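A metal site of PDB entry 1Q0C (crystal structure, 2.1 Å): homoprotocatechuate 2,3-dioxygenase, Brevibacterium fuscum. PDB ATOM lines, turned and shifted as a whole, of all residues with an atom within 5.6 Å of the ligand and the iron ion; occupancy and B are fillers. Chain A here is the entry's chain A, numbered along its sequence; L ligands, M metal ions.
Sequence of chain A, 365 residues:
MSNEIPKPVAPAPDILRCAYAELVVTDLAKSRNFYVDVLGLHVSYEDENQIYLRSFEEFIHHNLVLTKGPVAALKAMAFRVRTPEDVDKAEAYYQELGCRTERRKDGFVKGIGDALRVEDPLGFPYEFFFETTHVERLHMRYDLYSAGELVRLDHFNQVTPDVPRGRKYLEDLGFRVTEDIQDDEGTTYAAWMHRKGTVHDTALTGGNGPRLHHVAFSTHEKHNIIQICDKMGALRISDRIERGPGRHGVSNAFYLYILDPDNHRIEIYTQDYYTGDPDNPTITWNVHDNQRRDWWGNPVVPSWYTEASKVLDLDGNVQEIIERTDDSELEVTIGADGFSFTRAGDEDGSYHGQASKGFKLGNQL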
ATOM      1  N   HIS A 155     -19.989 -21.620  12.795  1.00  0.00           N
ATOM      2  CA  HIS A 155     -19.104 -22.806  12.820  1.00  0.00           C
ATOM      3  C   HIS A 155     -17.842 -22.667  12.005  1.00  0.00           C
ATOM      4  O   HIS A 155     -17.640 -21.696  11.254  1.00  0.00           O
ATOM      5  CB  HIS A 155     -19.842 -24.042  12.241  1.00  0.00           C
ATOM      6  CG  HIS A 155     -20.182 -23.924  10.763  1.00  0.00           C
ATOM      7  ND1 HIS A 155     -21.445 -23.592  10.309  1.00  0.00           N
ATOM      8  CD2 HIS A 155     -19.419 -24.110   9.655  1.00  0.00           C
ATOM      9  CE1 HIS A 155     -21.451 -23.599   8.975  1.00  0.00           C
ATOM     10  NE2 HIS A 155     -20.229 -23.899   8.556  1.00  0.00           N
ATOM     11  N   ASN A 157     -15.002 -25.288   9.656  1.00  0.00           N
ATOM     12  CA  ASN A 157     -14.950 -26.496   8.842  1.00  0.00           C
ATOM     13  C   ASN A 157     -13.450 -26.746   8.538  1.00  0.00           C
ATOM     14  O   ASN A 157     -12.804 -25.928   7.845  1.00  0.00           O
ATOM     15  CB  ASN A 157     -15.706 -26.317   7.547  1.00  0.00           C
ATOM     16  CG  ASN A 157     -15.829 -27.590   6.796  1.00  0.00           C
ATOM     17  OD1 ASN A 157     -14.837 -28.250   6.606  1.00  0.00           O
ATOM     18  ND2 ASN A 157     -17.037 -27.951   6.357  1.00  0.00           N
ATOM     19  N   TRP A 192     -20.208 -33.723  10.416  1.00  0.00           N
ATOM     20  CA  TRP A 192     -20.615 -32.429  10.970  1.00  0.00           C
ATOM     21  C   TRP A 192     -20.903 -32.664  12.416  1.00  0.00           C
ATOM     22  O   TRP A 192     -21.617 -33.611  12.740  1.00  0.00           O
ATOM     23  CB  TRP A 192     -21.851 -31.907  10.224  1.00  0.00           C
ATOM     24  CG  TRP A 192     -21.523 -31.369   8.850  1.00  0.00           C
ATOM     25  CD1 TRP A 192     -21.464 -30.066   8.508  1.00  0.00           C
ATOM     26  CD2 TRP A 192     -21.225 -32.113   7.659  1.00  0.00           C
ATOM     27  NE1 TRP A 192     -21.167 -29.933   7.174  1.00  0.00           N
ATOM     28  CE2 TRP A 192     -21.012 -31.177   6.616  1.00  0.00           C
ATOM     29  CE3 TRP A 192     -21.134 -33.479   7.358  1.00  0.00           C
ATOM     30  CZ2 TRP A 192     -20.709 -31.558   5.287  1.00  0.00           C
ATOM     31  CZ3 TRP A 192     -20.837 -33.870   6.062  1.00  0.00           C
ATOM     32  CH2 TRP A 192     -20.628 -32.899   5.023  1.00  0.00           C
ATOM     33  N   HIS A 200     -23.839 -27.858  13.413  1.00  0.00           N
ATOM     34  CA  HIS A 200     -22.418 -28.008  13.808  1.00  0.00           C
ATOM     35  C   HIS A 200     -21.701 -26.799  14.380  1.00  0.00           C
ATOM     36  O   HIS A 200     -22.164 -25.659  14.234  1.00  0.00           O
ATOM     37  CB  HIS A 200     -21.553 -28.534  12.662  1.00  0.00           C
ATOM     38  CG  HIS A 200     -21.600 -27.690  11.422  1.00  0.00           C
ATOM     39  ND1 HIS A 200     -22.761 -27.125  10.944  1.00  0.00           N
ATOM     40  CD2 HIS A 200     -20.645 -27.427  10.493  1.00  0.00           C
ATOM     41  CE1 HIS A 200     -22.525 -26.574   9.773  1.00  0.00           C
ATOM     42  NE2 HIS A 200     -21.254 -26.747   9.471  1.00  0.00           N
ATOM     43  N   HIS A 214     -13.164 -23.173   6.047  1.00  0.00           N
ATOM     44  CA  HIS A 214     -13.879 -21.893   6.166  1.00  0.00           C
ATOM     45  C   HIS A 214     -14.407 -21.592   7.561  1.00  0.00           C
ATOM     46  O   HIS A 214     -14.423 -22.441   8.455  1.00  0.00           O
ATOM     47  CB  HIS A 214     -15.030 -21.802   5.129  1.00  0.00           C
ATOM     48  CG  HIS A 214     -16.104 -22.841   5.291  1.00  0.00           C
ATOM     49  ND1 HIS A 214     -16.080 -24.044   4.609  1.00  0.00           N
ATOM     50  CD2 HIS A 214     -17.142 -22.911   6.147  1.00  0.00           C
ATOM     51  CE1 HIS A 214     -17.057 -24.811   5.061  1.00  0.00           C
ATOM     52  NE2 HIS A 214     -17.708 -24.146   5.991  1.00  0.00           N
ATOM     53  N   ALA A 216     -17.869 -19.784   9.229  1.00  0.00           N
ATOM     54  CA  ALA A 216     -19.223 -19.433   8.775  1.00  0.00           C
ATOM     55  C   ALA A 216     -19.970 -18.501   9.684  1.00  0.00           C
ATOM     56  O   ALA A 216     -19.952 -18.662  10.912  1.00  0.00           O
ATOM     57  CB  ALA A 216     -20.076 -20.686   8.606  1.00  0.00           C
ATOM     58  N   ARG A 243     -18.742 -20.019  -4.398  1.00  0.00           N
ATOM     59  CA  ARG A 243     -19.746 -21.033  -4.633  1.00  0.00           C
ATOM     60  C   ARG A 243     -21.080 -20.573  -4.020  1.00  0.00           C
ATOM     61  O   ARG A 243     -21.120 -20.059  -2.911  1.00  0.00           O
ATOM     62  CB  ARG A 243     -19.265 -22.356  -3.968  1.00  0.00           C
ATOM     63  CG  ARG A 243     -20.257 -23.467  -3.960  1.00  0.00           C
ATOM     64  CD  ARG A 243     -19.735 -24.707  -3.304  1.00  0.00           C
ATOM     65  NE  ARG A 243     -20.822 -25.671  -3.238  1.00  0.00           N
ATOM     66  CZ  ARG A 243     -20.987 -26.541  -2.251  1.00  0.00           C
ATOM     67  NH1 ARG A 243     -20.129 -26.573  -1.234  1.00  0.00           N
ATOM     68  NH2 ARG A 243     -22.048 -27.349  -2.260  1.00  0.00           N
ATOM     69  N   HIS A 248     -27.905 -26.204   0.881  1.00  0.00           N
ATOM     70  CA  HIS A 248     -27.073 -27.394   1.127  1.00  0.00           C
ATOM     71  C   HIS A 248     -27.989 -28.607   1.322  1.00  0.00           C
ATOM     72  O   HIS A 248     -29.115 -28.468   1.856  1.00  0.00           O
ATOM     73  CB  HIS A 248     -26.324 -27.283   2.469  1.00  0.00           C
ATOM     74  CG  HIS A 248     -25.087 -26.445   2.442  1.00  0.00           C
ATOM     75  ND1 HIS A 248     -24.092 -26.597   1.489  1.00  0.00           N
ATOM     76  CD2 HIS A 248     -24.637 -25.497   3.317  1.00  0.00           C
ATOM     77  CE1 HIS A 248     -23.079 -25.777   1.782  1.00  0.00           C
ATOM     78  NE2 HIS A 248     -23.387 -25.102   2.876  1.00  0.00           N
ATOM     79  N   GLY A 249     -27.529 -29.801   0.908  1.00  0.00           N
ATOM     80  CA  GLY A 249     -28.277 -31.021   1.195  1.00  0.00           C
ATOM     81  C   GLY A 249     -27.948 -31.246   2.668  1.00  0.00           C
ATOM     82  O   GLY A 249     -28.799 -31.091   3.533  1.00  0.00           O
ATOM     83  N   VAL A 250     -26.704 -31.596   2.965  1.00  0.00           N
ATOM     84  CA  VAL A 250     -26.269 -31.748   4.358  1.00  0.00           C
ATOM     85  C   VAL A 250     -26.535 -30.401   5.068  1.00  0.00           C
ATOM     86  O   VAL A 250     -26.161 -29.346   4.538  1.00  0.00           O
ATOM     87  CB  VAL A 250     -24.723 -32.046   4.467  1.00  0.00           C
ATOM     88  CG1 VAL A 250     -24.313 -32.179   5.935  1.00  0.00           C
ATOM     89  CG2 VAL A 250     -24.372 -33.328   3.775  1.00  0.00           C
ATOM     90  N   SER A 251     -27.164 -30.459   6.243  1.00  0.00           N
ATOM     91  CA  SER A 251     -27.498 -29.274   7.067  1.00  0.00           C
ATOM     92  C   SER A 251     -28.767 -28.559   6.646  1.00  0.00           C
ATOM     93  O   SER A 251     -29.366 -27.875   7.476  1.00  0.00           O
ATOM     94  CB  SER A 251     -26.371 -28.237   7.112  1.00  0.00           C
ATOM     95  OG  SER A 251     -26.454 -27.335   6.024  1.00  0.00           O
ATOM     96  N   TYR A 255     -26.895 -21.181   1.621  1.00  0.00           N
ATOM     97  CA  TYR A 255     -25.481 -20.784   1.823  1.00  0.00           C
ATOM     98  C   TYR A 255     -24.859 -19.997   0.697  1.00  0.00           C
ATOM     99  O   TYR A 255     -25.416 -19.895  -0.373  1.00  0.00           O
ATOM    100  CB  TYR A 255     -24.653 -22.079   2.005  1.00  0.00           C
ATOM    101  CG  TYR A 255     -24.477 -22.832   0.682  1.00  0.00           C
ATOM    102  CD1 TYR A 255     -23.452 -22.474  -0.216  1.00  0.00           C
ATOM    103  CD2 TYR A 255     -25.378 -23.828   0.288  1.00  0.00           C
ATOM    104  CE1 TYR A 255     -23.325 -23.100  -1.496  1.00  0.00           C
ATOM    105  CE2 TYR A 255     -25.263 -24.473  -0.995  1.00  0.00           C
ATOM    106  CZ  TYR A 255     -24.229 -24.098  -1.860  1.00  0.00           C
ATOM    107  OH  TYR A 255     -24.055 -24.716  -3.061  1.00  0.00           O
ATOM    108  N   TYR A 257     -20.482 -18.895  -0.342  1.00  0.00           N
ATOM    109  CA  TYR A 257     -19.047 -18.953  -0.027  1.00  0.00           C
ATOM    110  C   TYR A 257     -18.360 -17.868  -0.768  1.00  0.00           C
ATOM    111  O   TYR A 257     -18.489 -17.757  -1.991  1.00  0.00           O
ATOM    112  CB  TYR A 257     -18.377 -20.261  -0.441  1.00  0.00           C
ATOM    113  CG  TYR A 257     -18.842 -21.436   0.397  1.00  0.00           C
ATOM    114  CD1 TYR A 257     -18.300 -21.697   1.655  1.00  0.00           C
ATOM    115  CD2 TYR A 257     -19.847 -22.272  -0.090  1.00  0.00           C
ATOM    116  CE1 TYR A 257     -18.772 -22.767   2.432  1.00  0.00           C
ATOM    117  CE2 TYR A 257     -20.316 -23.337   0.671  1.00  0.00           C
ATOM    118  CZ  TYR A 257     -19.771 -23.593   1.912  1.00  0.00           C
ATOM    119  OH  TYR A 257     -20.237 -24.708   2.577  1.00  0.00           O
ATOM    120  N   GLU A 267     -18.074 -18.474   4.919  1.00  0.00           N
ATOM    121  CA  GLU A 267     -19.365 -18.952   4.432  1.00  0.00           C
ATOM    122  C   GLU A 267     -20.454 -18.145   5.123  1.00  0.00           C
ATOM    123  O   GLU A 267     -20.295 -17.807   6.308  1.00  0.00           O
ATOM    124  CB  GLU A 267     -19.602 -20.433   4.745  1.00  0.00           C
ATOM    125  CG  GLU A 267     -20.953 -20.895   4.245  1.00  0.00           C
ATOM    126  CD  GLU A 267     -21.313 -22.275   4.762  1.00  0.00           C
ATOM    127  OE1 GLU A 267     -20.699 -22.700   5.766  1.00  0.00           O
ATOM    128  OE2 GLU A 267     -22.214 -22.921   4.182  1.00  0.00           O
ATOM    129  N   TYR A 269     -24.467 -18.389   5.882  1.00  0.00           N
ATOM    130  CA  TYR A 269     -25.399 -19.499   6.038  1.00  0.00           C
ATOM    131  C   TYR A 269     -26.642 -19.080   6.798  1.00  0.00           C
ATOM    132  O   TYR A 269     -26.553 -18.201   7.659  1.00  0.00           O
ATOM    133  CB  TYR A 269     -24.574 -20.449   6.907  1.00  0.00           C
ATOM    134  CG  TYR A 269     -25.105 -21.716   7.469  1.00  0.00           C
ATOM    135  CD1 TYR A 269     -25.855 -21.748   8.671  1.00  0.00           C
ATOM    136  CD2 TYR A 269     -24.620 -22.941   6.939  1.00  0.00           C
ATOM    137  CE1 TYR A 269     -26.043 -23.002   9.329  1.00  0.00           C
ATOM    138  CE2 TYR A 269     -24.790 -24.148   7.554  1.00  0.00           C
ATOM    139  CZ  TYR A 269     -25.493 -24.201   8.741  1.00  0.00           C
ATOM    140  OH  TYR A 269     -25.518 -25.425   9.349  1.00  0.00           O
ATOM    141  N   ARG A 292     -26.356 -34.352  -1.973  1.00  0.00           N
ATOM    142  CA  ARG A 292     -25.795 -34.180  -0.637  1.00  0.00           C
ATOM    143  C   ARG A 292     -25.116 -32.829  -0.367  1.00  0.00           C
ATOM    144  O   ARG A 292     -25.142 -32.338   0.756  1.00  0.00           O
ATOM    145  CB  ARG A 292     -24.780 -35.300  -0.314  1.00  0.00           C
ATOM    146  CG  ARG A 292     -23.569 -35.330  -1.204  1.00  0.00           C
ATOM    147  CD  ARG A 292     -22.672 -36.574  -0.882  1.00  0.00           C
ATOM    148  NE  ARG A 292     -21.342 -36.396  -1.449  1.00  0.00           N
ATOM    149  CZ  ARG A 292     -21.079 -36.363  -2.754  1.00  0.00           C
ATOM    150  NH1 ARG A 292     -22.069 -36.505  -3.654  1.00  0.00           N
ATOM    151  NH2 ARG A 292     -19.842 -36.099  -3.171  1.00  0.00           N
ATOM    152  N   ARG A 293     -24.502 -32.221  -1.366  1.00  0.00           N
ATOM    153  CA  ARG A 293     -23.804 -30.946  -1.072  1.00  0.00           C
ATOM    154  C   ARG A 293     -24.703 -29.815  -1.487  1.00  0.00           C
ATOM    155  O   ARG A 293     -25.105 -28.996  -0.643  1.00  0.00           O
ATOM    156  CB  ARG A 293     -22.454 -30.856  -1.805  1.00  0.00           C
ATOM    157  CG  ARG A 293     -21.674 -32.166  -1.767  1.00  0.00           C
ATOM    158  CD  ARG A 293     -20.158 -32.063  -1.483  1.00  0.00           C
ATOM    159  NE  ARG A 293     -19.887 -31.706  -0.103  1.00  0.00           N
ATOM    160  CZ  ARG A 293     -18.778 -32.017   0.542  1.00  0.00           C
ATOM    161  NH1 ARG A 293     -17.827 -32.714  -0.079  1.00  0.00           N
ATOM    162  NH2 ARG A 293     -18.586 -31.595   1.792  1.00  0.00           N
ATOM    163  N   ASP A 294     -25.033 -29.771  -2.758  1.00  0.00           N
ATOM    164  CA  ASP A 294     -25.942 -28.756  -3.204  1.00  0.00           C
ATOM    165  C   ASP A 294     -27.231 -29.484  -3.572  1.00  0.00           C
ATOM    166  O   ASP A 294     -27.303 -30.274  -4.556  1.00  0.00           O
ATOM    167  CB  ASP A 294     -25.343 -27.987  -4.377  1.00  0.00           C
ATOM    168  CG  ASP A 294     -26.241 -26.869  -4.832  1.00  0.00           C
ATOM    169  OD1 ASP A 294     -27.157 -27.150  -5.638  1.00  0.00           O
ATOM    170  OD2 ASP A 294     -26.053 -25.719  -4.353  1.00  0.00           O
ATOM    171  N   VAL A 300     -20.281 -28.526  -8.107  1.00  0.00           N
ATOM    172  CA  VAL A 300     -19.428 -27.988  -7.017  1.00  0.00           C
ATOM    173  C   VAL A 300     -18.086 -27.448  -7.566  1.00  0.00           C
ATOM    174  O   VAL A 300     -17.260 -28.201  -8.076  1.00  0.00           O
ATOM    175  CB  VAL A 300     -19.072 -29.094  -5.945  1.00  0.00           C
ATOM    176  CG1 VAL A 300     -18.389 -28.467  -4.744  1.00  0.00           C
ATOM    177  CG2 VAL A 300     -20.310 -29.835  -5.475  1.00  0.00           C
ATOM    178  N   TRP A 304     -13.250 -25.169  -4.552  1.00  0.00           N
ATOM    179  CA  TRP A 304     -13.897 -25.401  -3.282  1.00  0.00           C
ATOM    180  C   TRP A 304     -13.305 -26.656  -2.635  1.00  0.00           C
ATOM    181  O   TRP A 304     -13.275 -26.780  -1.417  1.00  0.00           O
ATOM    182  CB  TRP A 304     -15.433 -25.530  -3.455  1.00  0.00           C
ATOM    183  CG  TRP A 304     -16.229 -25.387  -2.157  1.00  0.00           C
ATOM    184  CD1 TRP A 304     -16.662 -24.216  -1.566  1.00  0.00           C
ATOM    185  CD2 TRP A 304     -16.578 -26.431  -1.261  1.00  0.00           C
ATOM    186  NE1 TRP A 304     -17.241 -24.467  -0.356  1.00  0.00           N
ATOM    187  CE2 TRP A 304     -17.208 -25.825  -0.136  1.00  0.00           C
ATOM    188  CE3 TRP A 304     -16.420 -27.822  -1.273  1.00  0.00           C
ATOM    189  CZ2 TRP A 304     -17.661 -26.560   0.948  1.00  0.00           C
ATOM    190  CZ3 TRP A 304     -16.889 -28.566  -0.202  1.00  0.00           C
ATOM    191  CH2 TRP A 304     -17.500 -27.932   0.893  1.00  0.00           C
ATOM    192  N   TYR A 305     -12.822 -27.594  -3.457  1.00  0.00           N
ATOM    193  CA  TYR A 305     -12.260 -28.834  -2.904  1.00  0.00           C
ATOM    194  C   TYR A 305     -10.755 -28.774  -2.703  1.00  0.00           C
ATOM    195  O   TYR A 305     -10.199 -29.438  -1.835  1.00  0.00           O
ATOM    196  CB  TYR A 305     -12.579 -30.024  -3.815  1.00  0.00           C
ATOM    197  CG  TYR A 305     -14.005 -30.470  -3.752  1.00  0.00           C
ATOM    198  CD1 TYR A 305     -14.522 -31.013  -2.572  1.00  0.00           C
ATOM    199  CD2 TYR A 305     -14.828 -30.402  -4.868  1.00  0.00           C
ATOM    200  CE1 TYR A 305     -15.831 -31.487  -2.507  1.00  0.00           C
ATOM    201  CE2 TYR A 305     -16.150 -30.877  -4.817  1.00  0.00           C
ATOM    202  CZ  TYR A 305     -16.630 -31.419  -3.629  1.00  0.00           C
ATOM    203  OH  TYR A 305     -17.923 -31.884  -3.552  1.00  0.00           O
HETATM  204  C1  LIG L   1     -21.846 -28.704   3.391  1.00  0.00           C
HETATM  205  C2  LIG L   1     -20.720 -27.843   3.651  1.00  0.00           C
HETATM  206  C3  LIG L   1     -20.774 -26.885   4.693  1.00  0.00           C
HETATM  207  C4  LIG L   1     -21.954 -26.779   5.503  1.00  0.00           C
HETATM  208  C5  LIG L   1     -23.073 -27.636   5.264  1.00  0.00           C
HETATM  209  C6  LIG L   1     -23.009 -28.593   4.199  1.00  0.00           C
HETATM  210  C7  LIG L   1     -21.669 -29.633   2.253  1.00  0.00           C
HETATM  211  C8  LIG L   1     -21.587 -28.933   0.925  1.00  0.00           C
HETATM  212  O1  LIG L   1     -20.526 -28.985   0.275  1.00  0.00           O
HETATM  213  O2  LIG L   1     -22.471 -28.245   0.362  1.00  0.00           O
HETATM  214  O3  LIG L   1     -19.825 -25.963   5.110  1.00  0.00           O
HETATM  215  O4  LIG L   1     -21.819 -25.781   6.484  1.00  0.00           O
HETATM  216 FE    FE M   1     -19.912 -24.509   6.425  1.00  0.00          FE
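ND1 of His 248 is in hydrogen-bond range of O2 of the ligand (2.6 Å). An oxygen (O2) of the ligand is in salt-bridge range of the guanidinium group of Arg 243 (2.8 Å). An oxygen (O2) of the ligand sits close to the backbone carbonyl oxygen (O) of Arg 293, at 2.9 Å. The guanidinium group (NE) of Arg 293 is in salt-bridge range of an oxygen (O1) of the ligand, at 2.8 Å. The side-chain hydroxyl (OH) of Tyr 257 lies close to an oxygen (O3) of the ligand, 2.9 Å away. An oxygen (O4) of the ligand lies close to a ring nitrogen (NE2) of His 200 (3.2 Å).
A ring nitrogen (NE2) of His 248 sits at hydrogen-bond distance from the side-chain carboxylate (OE2) of Glu 267, 2.8 Å away. The side-chain carboxylate (OE2) of Glu 267 lies within hydrogen-bond range of the side-chain hydroxyl (OH) of Tyr 257 (3.1 Å). N of Ala 216 sits at hydrogen-bond distance from O of His 155, 2.8 Å away. The backbone carbonyl oxygen (O) of Arg 293 sits close to a ring nitrogen (ND1) of His 248, 3.4 Å away. A ring nitrogen (NE2) of His 248 lies close to the side-chain hydroxyl (OH) of Tyr 257, 3.2 Å away. The backbone NH (N) of Tyr 257 lies within hydrogen-bond range of the backbone carbonyl oxygen (O) of Arg 243. NE of Arg 243 lies within hydrogen-bond range of OH of Tyr 255, at 3.4 Å. O of Arg 292 lies within hydrogen-bond range of N of Val 250, 2.8 Å away.
Merely in contact with the ligand: Asn 157, Trp 192, Val 250, Ser 251, Tyr 269 and Trp 304. Hydrophobic or aromatic side chains that line the ligand: His 155, Trp 192, His 200, His 214, His 248, Val 250, Tyr 257, Tyr 269 and Trp 304. The nearest printed residue that does not touch the ligand is Asp 294 (4.3 Å).
Tyr 257 touches the iron ion (OH to FE, 3.9 Å). Within 4 Å of the iron ion: His 155, His 214, Tyr 257 and Glu 267.
The iron ion is bound by O3 of the ligand. OE1 of Glu 267 is bound to the iron ion (2.1 Å). NE2 of His 155 binds the iron ion. NE2 of His 214 is bound to the iron ion, at 2.3 Å. The iron ion is bound by an oxygen (O4) of the ligand. The iron ion has five donor atoms within binding distance.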
